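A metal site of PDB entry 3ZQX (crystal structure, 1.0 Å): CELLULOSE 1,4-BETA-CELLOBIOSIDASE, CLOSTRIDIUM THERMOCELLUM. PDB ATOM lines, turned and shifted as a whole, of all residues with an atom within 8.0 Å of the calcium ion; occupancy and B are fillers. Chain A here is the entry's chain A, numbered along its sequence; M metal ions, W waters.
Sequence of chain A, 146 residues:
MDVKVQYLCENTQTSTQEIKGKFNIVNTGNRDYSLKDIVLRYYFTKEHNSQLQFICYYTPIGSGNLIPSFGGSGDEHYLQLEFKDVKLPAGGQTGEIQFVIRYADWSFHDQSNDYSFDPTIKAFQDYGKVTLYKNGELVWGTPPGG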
ATOM      1  N   THR A  14     -22.053  -7.276 -25.197  1.00  0.00           N
ATOM      2  CA  THR A  14     -22.352  -5.859 -24.982  1.00  0.00           C
ATOM      3  C   THR A  14     -22.793  -5.640 -23.535  1.00  0.00           C
ATOM      4  O   THR A  14     -22.238  -4.806 -22.805  1.00  0.00           O
ATOM      5  CB  THR A  14     -23.467  -5.379 -25.952  1.00  0.00           C
ATOM      6  OG1 THR A  14     -23.001  -5.488 -27.308  1.00  0.00           O
ATOM      7  CG2 THR A  14     -23.842  -3.930 -25.676  1.00  0.00           C
ATOM      8  N   ILE A  19     -16.721  -6.565 -17.239  1.00  0.00           N
ATOM      9  CA  ILE A  19     -15.722  -6.332 -18.267  1.00  0.00           C
ATOM     10  C   ILE A  19     -14.580  -7.289 -17.947  1.00  0.00           C
ATOM     11  O   ILE A  19     -14.233  -7.429 -16.779  1.00  0.00           O
ATOM     12  CB  ILE A  19     -15.209  -4.871 -18.229  1.00  0.00           C
ATOM     13  CG1 ILE A  19     -16.349  -3.889 -18.510  1.00  0.00           C
ATOM     14  CG2 ILE A  19     -14.045  -4.685 -19.193  1.00  0.00           C
ATOM     15  CD1 ILE A  19     -15.975  -2.427 -18.286  1.00  0.00           C
ATOM     16  N   TYR A  43     -10.105   2.601 -20.817  1.00  0.00           N
ATOM     17  CA  TYR A  43     -11.175   3.595 -20.873  1.00  0.00           C
ATOM     18  C   TYR A  43     -12.533   2.951 -21.087  1.00  0.00           C
ATOM     19  O   TYR A  43     -12.725   2.161 -22.013  1.00  0.00           O
ATOM     20  CB  TYR A  43     -10.876   4.606 -21.992  1.00  0.00           C
ATOM     21  CG  TYR A  43      -9.579   5.334 -21.747  1.00  0.00           C
ATOM     22  CD1 TYR A  43      -9.539   6.453 -20.931  1.00  0.00           C
ATOM     23  CD2 TYR A  43      -8.373   4.861 -22.280  1.00  0.00           C
ATOM     24  CE1 TYR A  43      -8.340   7.100 -20.668  1.00  0.00           C
ATOM     25  CE2 TYR A  43      -7.179   5.505 -22.025  1.00  0.00           C
ATOM     26  CZ  TYR A  43      -7.158   6.628 -21.223  1.00  0.00           C
ATOM     27  OH  TYR A  43      -5.958   7.239 -20.971  1.00  0.00           O
ATOM     28  N   PHE A  44     -13.476   3.285 -20.205  1.00  0.00           N
ATOM     29  CA  PHE A  44     -14.828   2.782 -20.329  1.00  0.00           C
ATOM     30  C   PHE A  44     -15.772   3.776 -19.680  1.00  0.00           C
ATOM     31  O   PHE A  44     -15.382   4.488 -18.749  1.00  0.00           O
ATOM     32  CB  PHE A  44     -14.967   1.391 -19.696  1.00  0.00           C
ATOM     33  CG  PHE A  44     -14.964   1.378 -18.188  1.00  0.00           C
ATOM     34  CD1 PHE A  44     -13.783   1.440 -17.460  1.00  0.00           C
ATOM     35  CD2 PHE A  44     -16.161   1.271 -17.495  1.00  0.00           C
ATOM     36  CE1 PHE A  44     -13.802   1.415 -16.070  1.00  0.00           C
ATOM     37  CE2 PHE A  44     -16.188   1.247 -16.100  1.00  0.00           C
ATOM     38  CZ  PHE A  44     -14.995   1.293 -15.386  1.00  0.00           C
ATOM     39  N   THR A  45     -16.999   3.794 -20.163  1.00  0.00           N
ATOM     40  CA  THR A  45     -18.021   4.663 -19.614  1.00  0.00           C
ATOM     41  C   THR A  45     -18.810   3.911 -18.564  1.00  0.00           C
ATOM     42  O   THR A  45     -19.266   2.786 -18.794  1.00  0.00           O
ATOM     43  CB  THR A  45     -18.978   5.157 -20.701  1.00  0.00           C
ATOM     44  OG1 THR A  45     -19.410   4.043 -21.474  1.00  0.00           O
ATOM     45  CG2 THR A  45     -18.293   6.184 -21.609  1.00  0.00           C
ATOM     46  N   LYS A  46     -18.976   4.525 -17.394  1.00  0.00           N
ATOM     47  CA  LYS A  46     -19.729   3.884 -16.335  1.00  0.00           C
ATOM     48  C   LYS A  46     -21.218   4.203 -16.448  1.00  0.00           C
ATOM     49  O   LYS A  46     -21.610   5.362 -16.546  1.00  0.00           O
ATOM     50  CB  LYS A  46     -19.175   4.207 -14.944  1.00  0.00           C
ATOM     51  CG  LYS A  46     -19.144   5.654 -14.561  1.00  0.00           C
ATOM     52  CD  LYS A  46     -18.681   5.788 -13.126  1.00  0.00           C
ATOM     53  CE  LYS A  46     -18.651   7.229 -12.703  1.00  0.00           C
ATOM     54  NZ  LYS A  46     -18.076   7.426 -11.337  1.00  0.00           N
ATOM     55  N   GLU A  47     -22.038   3.155 -16.443  1.00  0.00           N
ATOM     56  CA  GLU A  47     -23.485   3.278 -16.542  1.00  0.00           C
ATOM     57  C   GLU A  47     -24.188   3.403 -15.181  1.00  0.00           C
ATOM     58  O   GLU A  47     -25.365   3.747 -15.138  1.00  0.00           O
ATOM     59  CB  GLU A  47     -24.063   2.079 -17.301  1.00  0.00           C
ATOM     60  CG  GLU A  47     -24.000   2.175 -18.821  1.00  0.00           C
ATOM     61  CD  GLU A  47     -22.605   2.035 -19.392  1.00  0.00           C
ATOM     62  OE1 GLU A  47     -21.913   1.034 -19.096  1.00  0.00           O
ATOM     63  OE2 GLU A  47     -22.197   2.921 -20.169  1.00  0.00           O
ATOM     64  N   HIS A  48     -23.478   3.147 -14.095  1.00  0.00           N
ATOM     65  CA  HIS A  48     -24.107   3.153 -12.771  1.00  0.00           C
ATOM     66  C   HIS A  48     -23.238   3.822 -11.737  1.00  0.00           C
ATOM     67  O   HIS A  48     -22.032   3.931 -11.914  1.00  0.00           O
ATOM     68  CB  HIS A  48     -24.419   1.724 -12.312  1.00  0.00           C
ATOM     69  CG  HIS A  48     -25.191   0.929 -13.320  1.00  0.00           C
ATOM     70  ND1 HIS A  48     -26.563   1.005 -13.435  1.00  0.00           N
ATOM     71  CD2 HIS A  48     -24.770   0.046 -14.257  1.00  0.00           C
ATOM     72  CE1 HIS A  48     -26.955   0.194 -14.401  1.00  0.00           C
ATOM     73  NE2 HIS A  48     -25.900  -0.395 -14.918  1.00  0.00           N
ATOM     74  N   HIS A  77     -13.561   8.570 -18.720  1.00  0.00           N
ATOM     75  CA  HIS A  77     -13.498   7.683 -17.553  1.00  0.00           C
ATOM     76  C   HIS A  77     -12.643   6.443 -17.825  1.00  0.00           C
ATOM     77  O   HIS A  77     -12.586   5.936 -18.956  1.00  0.00           O
ATOM     78  CB  HIS A  77     -14.926   7.304 -17.168  1.00  0.00           C
ATOM     79  CG  HIS A  77     -15.024   6.497 -15.920  1.00  0.00           C
ATOM     80  ND1 HIS A  77     -15.154   5.126 -15.921  1.00  0.00           N
ATOM     81  CD2 HIS A  77     -14.996   6.869 -14.615  1.00  0.00           C
ATOM     82  CE1 HIS A  77     -15.208   4.684 -14.670  1.00  0.00           C
ATOM     83  NE2 HIS A  77     -15.122   5.729 -13.852  1.00  0.00           N
ATOM     84  N   TYR A 103     -19.387  -4.111 -10.724  1.00  0.00           N
ATOM     85  CA  TYR A 103     -19.990  -3.277  -9.703  1.00  0.00           C
ATOM     86  C   TYR A 103     -20.228  -4.049  -8.405  1.00  0.00           C
ATOM     87  O   TYR A 103     -20.531  -5.246  -8.441  1.00  0.00           O
ATOM     88  CB  TYR A 103     -21.327  -2.743 -10.195  1.00  0.00           C
ATOM     89  CG  TYR A 103     -21.218  -1.700 -11.269  1.00  0.00           C
ATOM     90  CD1 TYR A 103     -20.967  -0.386 -10.948  1.00  0.00           C
ATOM     91  CD2 TYR A 103     -21.388  -2.026 -12.614  1.00  0.00           C
ATOM     92  CE1 TYR A 103     -20.873   0.587 -11.923  1.00  0.00           C
ATOM     93  CE2 TYR A 103     -21.299  -1.066 -13.595  1.00  0.00           C
ATOM     94  CZ  TYR A 103     -21.037   0.244 -13.253  1.00  0.00           C
ATOM     95  OH  TYR A 103     -20.954   1.241 -14.194  1.00  0.00           O
ATOM     96  N   PHE A 108     -25.245  -4.235 -14.529  1.00  0.00           N
ATOM     97  CA  PHE A 108     -24.747  -4.511 -15.877  1.00  0.00           C
ATOM     98  C   PHE A 108     -24.048  -3.321 -16.521  1.00  0.00           C
ATOM     99  O   PHE A 108     -24.591  -2.204 -16.545  1.00  0.00           O
ATOM    100  CB  PHE A 108     -25.890  -4.942 -16.795  1.00  0.00           C
ATOM    101  CG  PHE A 108     -26.404  -6.330 -16.524  1.00  0.00           C
ATOM    102  CD1 PHE A 108     -27.300  -6.570 -15.496  1.00  0.00           C
ATOM    103  CD2 PHE A 108     -25.985  -7.398 -17.301  1.00  0.00           C
ATOM    104  CE1 PHE A 108     -27.771  -7.838 -15.250  1.00  0.00           C
ATOM    105  CE2 PHE A 108     -26.475  -8.671 -17.066  1.00  0.00           C
ATOM    106  CZ  PHE A 108     -27.357  -8.891 -16.041  1.00  0.00           C
ATOM    107  N   HIS A 109     -22.871  -3.568 -17.075  1.00  0.00           N
ATOM    108  CA  HIS A 109     -22.235  -2.644 -17.997  1.00  0.00           C
ATOM    109  C   HIS A 109     -22.887  -2.684 -19.364  1.00  0.00           C
ATOM    110  O   HIS A 109     -23.454  -3.696 -19.768  1.00  0.00           O
ATOM    111  CB  HIS A 109     -20.792  -3.072 -18.285  1.00  0.00           C
ATOM    112  CG  HIS A 109     -19.884  -3.095 -17.104  1.00  0.00           C
ATOM    113  ND1 HIS A 109     -19.292  -1.956 -16.592  1.00  0.00           N
ATOM    114  CD2 HIS A 109     -19.396  -4.129 -16.395  1.00  0.00           C
ATOM    115  CE1 HIS A 109     -18.494  -2.295 -15.591  1.00  0.00           C
ATOM    116  NE2 HIS A 109     -18.538  -3.613 -15.456  1.00  0.00           N
ATOM    117  N   ASP A 110     -22.741  -1.587 -20.098  1.00  0.00           N
ATOM    118  CA  ASP A 110     -22.874  -1.578 -21.548  1.00  0.00           C
ATOM    119  C   ASP A 110     -21.469  -1.364 -22.089  1.00  0.00           C
ATOM    120  O   ASP A 110     -20.891  -0.298 -21.912  1.00  0.00           O
ATOM    121  CB  ASP A 110     -23.787  -0.429 -21.974  1.00  0.00           C
ATOM    122  CG  ASP A 110     -23.943  -0.303 -23.481  1.00  0.00           C
ATOM    123  OD1 ASP A 110     -23.276  -1.025 -24.237  1.00  0.00           O
ATOM    124  OD2 ASP A 110     -24.742   0.552 -23.900  1.00  0.00           O
ATOM    125  N   GLN A 111     -20.887  -2.372 -22.717  1.00  0.00           N
ATOM    126  CA  GLN A 111     -19.533  -2.242 -23.219  1.00  0.00           C
ATOM    127  C   GLN A 111     -19.464  -1.548 -24.567  1.00  0.00           C
ATOM    128  O   GLN A 111     -18.379  -1.151 -24.992  1.00  0.00           O
ATOM    129  CB  GLN A 111     -18.851  -3.614 -23.344  1.00  0.00           C
ATOM    130  CG  GLN A 111     -18.757  -4.389 -22.053  1.00  0.00           C
ATOM    131  CD  GLN A 111     -17.692  -5.453 -22.129  1.00  0.00           C
ATOM    132  OE1 GLN A 111     -16.520  -5.200 -21.831  1.00  0.00           O
ATOM    133  NE2 GLN A 111     -18.075  -6.663 -22.533  1.00  0.00           N
ATOM    134  N   SER A 112     -20.602  -1.397 -25.244  1.00  0.00           N
ATOM    135  CA  SER A 112     -20.583  -0.870 -26.607  1.00  0.00           C
ATOM    136  C   SER A 112     -20.160   0.579 -26.707  1.00  0.00           C
ATOM    137  O   SER A 112     -19.778   1.034 -27.747  1.00  0.00           O
ATOM    138  CB  SER A 112     -21.937  -1.103 -27.321  1.00  0.00           C
ATOM    139  OG  SER A 112     -22.912  -0.275 -26.799  1.00  0.00           O
ATOM    140  N   ASN A 113     -20.245   1.274 -25.584  1.00  0.00           N
ATOM    141  CA  ASN A 113     -19.836   2.653 -25.499  1.00  0.00           C
ATOM    142  C   ASN A 113     -18.538   2.856 -24.688  1.00  0.00           C
ATOM    143  O   ASN A 113     -18.342   3.898 -24.088  1.00  0.00           O
ATOM    144  CB  ASN A 113     -20.972   3.523 -24.967  1.00  0.00           C
ATOM    145  CG  ASN A 113     -21.399   3.112 -23.605  1.00  0.00           C
ATOM    146  OD1 ASN A 113     -20.795   2.225 -23.026  1.00  0.00           O
ATOM    147  ND2 ASN A 113     -22.412   3.768 -23.054  1.00  0.00           N
ATOM    148  N   ASP A 114     -17.696   1.821 -24.696  1.00  0.00           N
ATOM    149  CA  ASP A 114     -16.422   1.860 -23.980  1.00  0.00           C
ATOM    150  C   ASP A 114     -15.279   1.962 -24.998  1.00  0.00           C
ATOM    151  O   ASP A 114     -15.116   1.105 -25.845  1.00  0.00           O
ATOM    152  CB  ASP A 114     -16.203   0.602 -23.163  1.00  0.00           C
ATOM    153  CG  ASP A 114     -17.190   0.476 -22.023  1.00  0.00           C
ATOM    154  OD1 ASP A 114     -17.903   1.443 -21.720  1.00  0.00           O
ATOM    155  OD2 ASP A 114     -17.232  -0.606 -21.398  1.00  0.00           O
ATOM    156  N   TYR A 115     -14.504   3.032 -24.884  1.00  0.00           N
ATOM    157  CA  TYR A 115     -13.433   3.296 -25.833  1.00  0.00           C
ATOM    158  C   TYR A 115     -12.444   2.150 -25.978  1.00  0.00           C
ATOM    159  O   TYR A 115     -12.013   1.826 -27.078  1.00  0.00           O
ATOM    160  CB  TYR A 115     -12.721   4.579 -25.402  1.00  0.00           C
ATOM    161  CG  TYR A 115     -11.506   4.963 -26.214  1.00  0.00           C
ATOM    162  CD1 TYR A 115     -11.640   5.708 -27.381  1.00  0.00           C
ATOM    163  CD2 TYR A 115     -10.223   4.665 -25.770  1.00  0.00           C
ATOM    164  CE1 TYR A 115     -10.522   6.103 -28.100  1.00  0.00           C
ATOM    165  CE2 TYR A 115      -9.109   5.064 -26.476  1.00  0.00           C
ATOM    166  CZ  TYR A 115      -9.261   5.777 -27.643  1.00  0.00           C
ATOM    167  OH  TYR A 115      -8.170   6.187 -28.375  1.00  0.00           O
ATOM    168  N   PHE A 117     -12.835  -1.100 -25.327  1.00  0.00           N
ATOM    169  CA  PHE A 117     -13.396  -2.426 -25.599  1.00  0.00           C
ATOM    170  C   PHE A 117     -13.229  -2.820 -27.066  1.00  0.00           C
ATOM    171  O   PHE A 117     -13.616  -2.059 -27.943  1.00  0.00           O
ATOM    172  CB  PHE A 117     -14.888  -2.365 -25.260  1.00  0.00           C
ATOM    173  CG  PHE A 117     -15.692  -3.596 -25.603  1.00  0.00           C
ATOM    174  CD1 PHE A 117     -15.428  -4.824 -25.025  1.00  0.00           C
ATOM    175  CD2 PHE A 117     -16.784  -3.488 -26.454  1.00  0.00           C
ATOM    176  CE1 PHE A 117     -16.202  -5.927 -25.314  1.00  0.00           C
ATOM    177  CE2 PHE A 117     -17.567  -4.580 -26.741  1.00  0.00           C
ATOM    178  CZ  PHE A 117     -17.280  -5.808 -26.165  1.00  0.00           C
HETATM  179 CA    CA M   1     -20.100   1.661 -20.764  1.00  0.00          CA
HETATM  180  O   HOH W   1     -19.098  -0.268 -19.490  1.00  0.00           O
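N of Glu 47 is in hydrogen-bond range of OH of Tyr 103 (3.1 Å). OD1 of Asp 110 lies within hydrogen-bond range of OG of Ser 112, 2.7 Å away.
Along chain A the residues within 4 Å of the calcium ion span positions 45 to 114.
The calcium ion is bound by the backbone carbonyl oxygen (O) of Asp 110, the side-chain carboxylate (OD1) of Asp 114, the backbone carbonyl oxygen (O) of Thr 45, the side-chain amide oxygen (OD1) of Asn 113, the side-chain carboxylate (OE2) of Glu 47, water W1, the side-chain carboxylate (OE1) of Glu 47 and the side-chain hydroxyl (OG1) of Thr 45. The calcium ion has eight donor atoms within binding distance.
Water W1 lies within hydrogen-bond range of OD2 of Asp 114 (2.7 Å) and ND1 of His 109 (3.4 Å).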
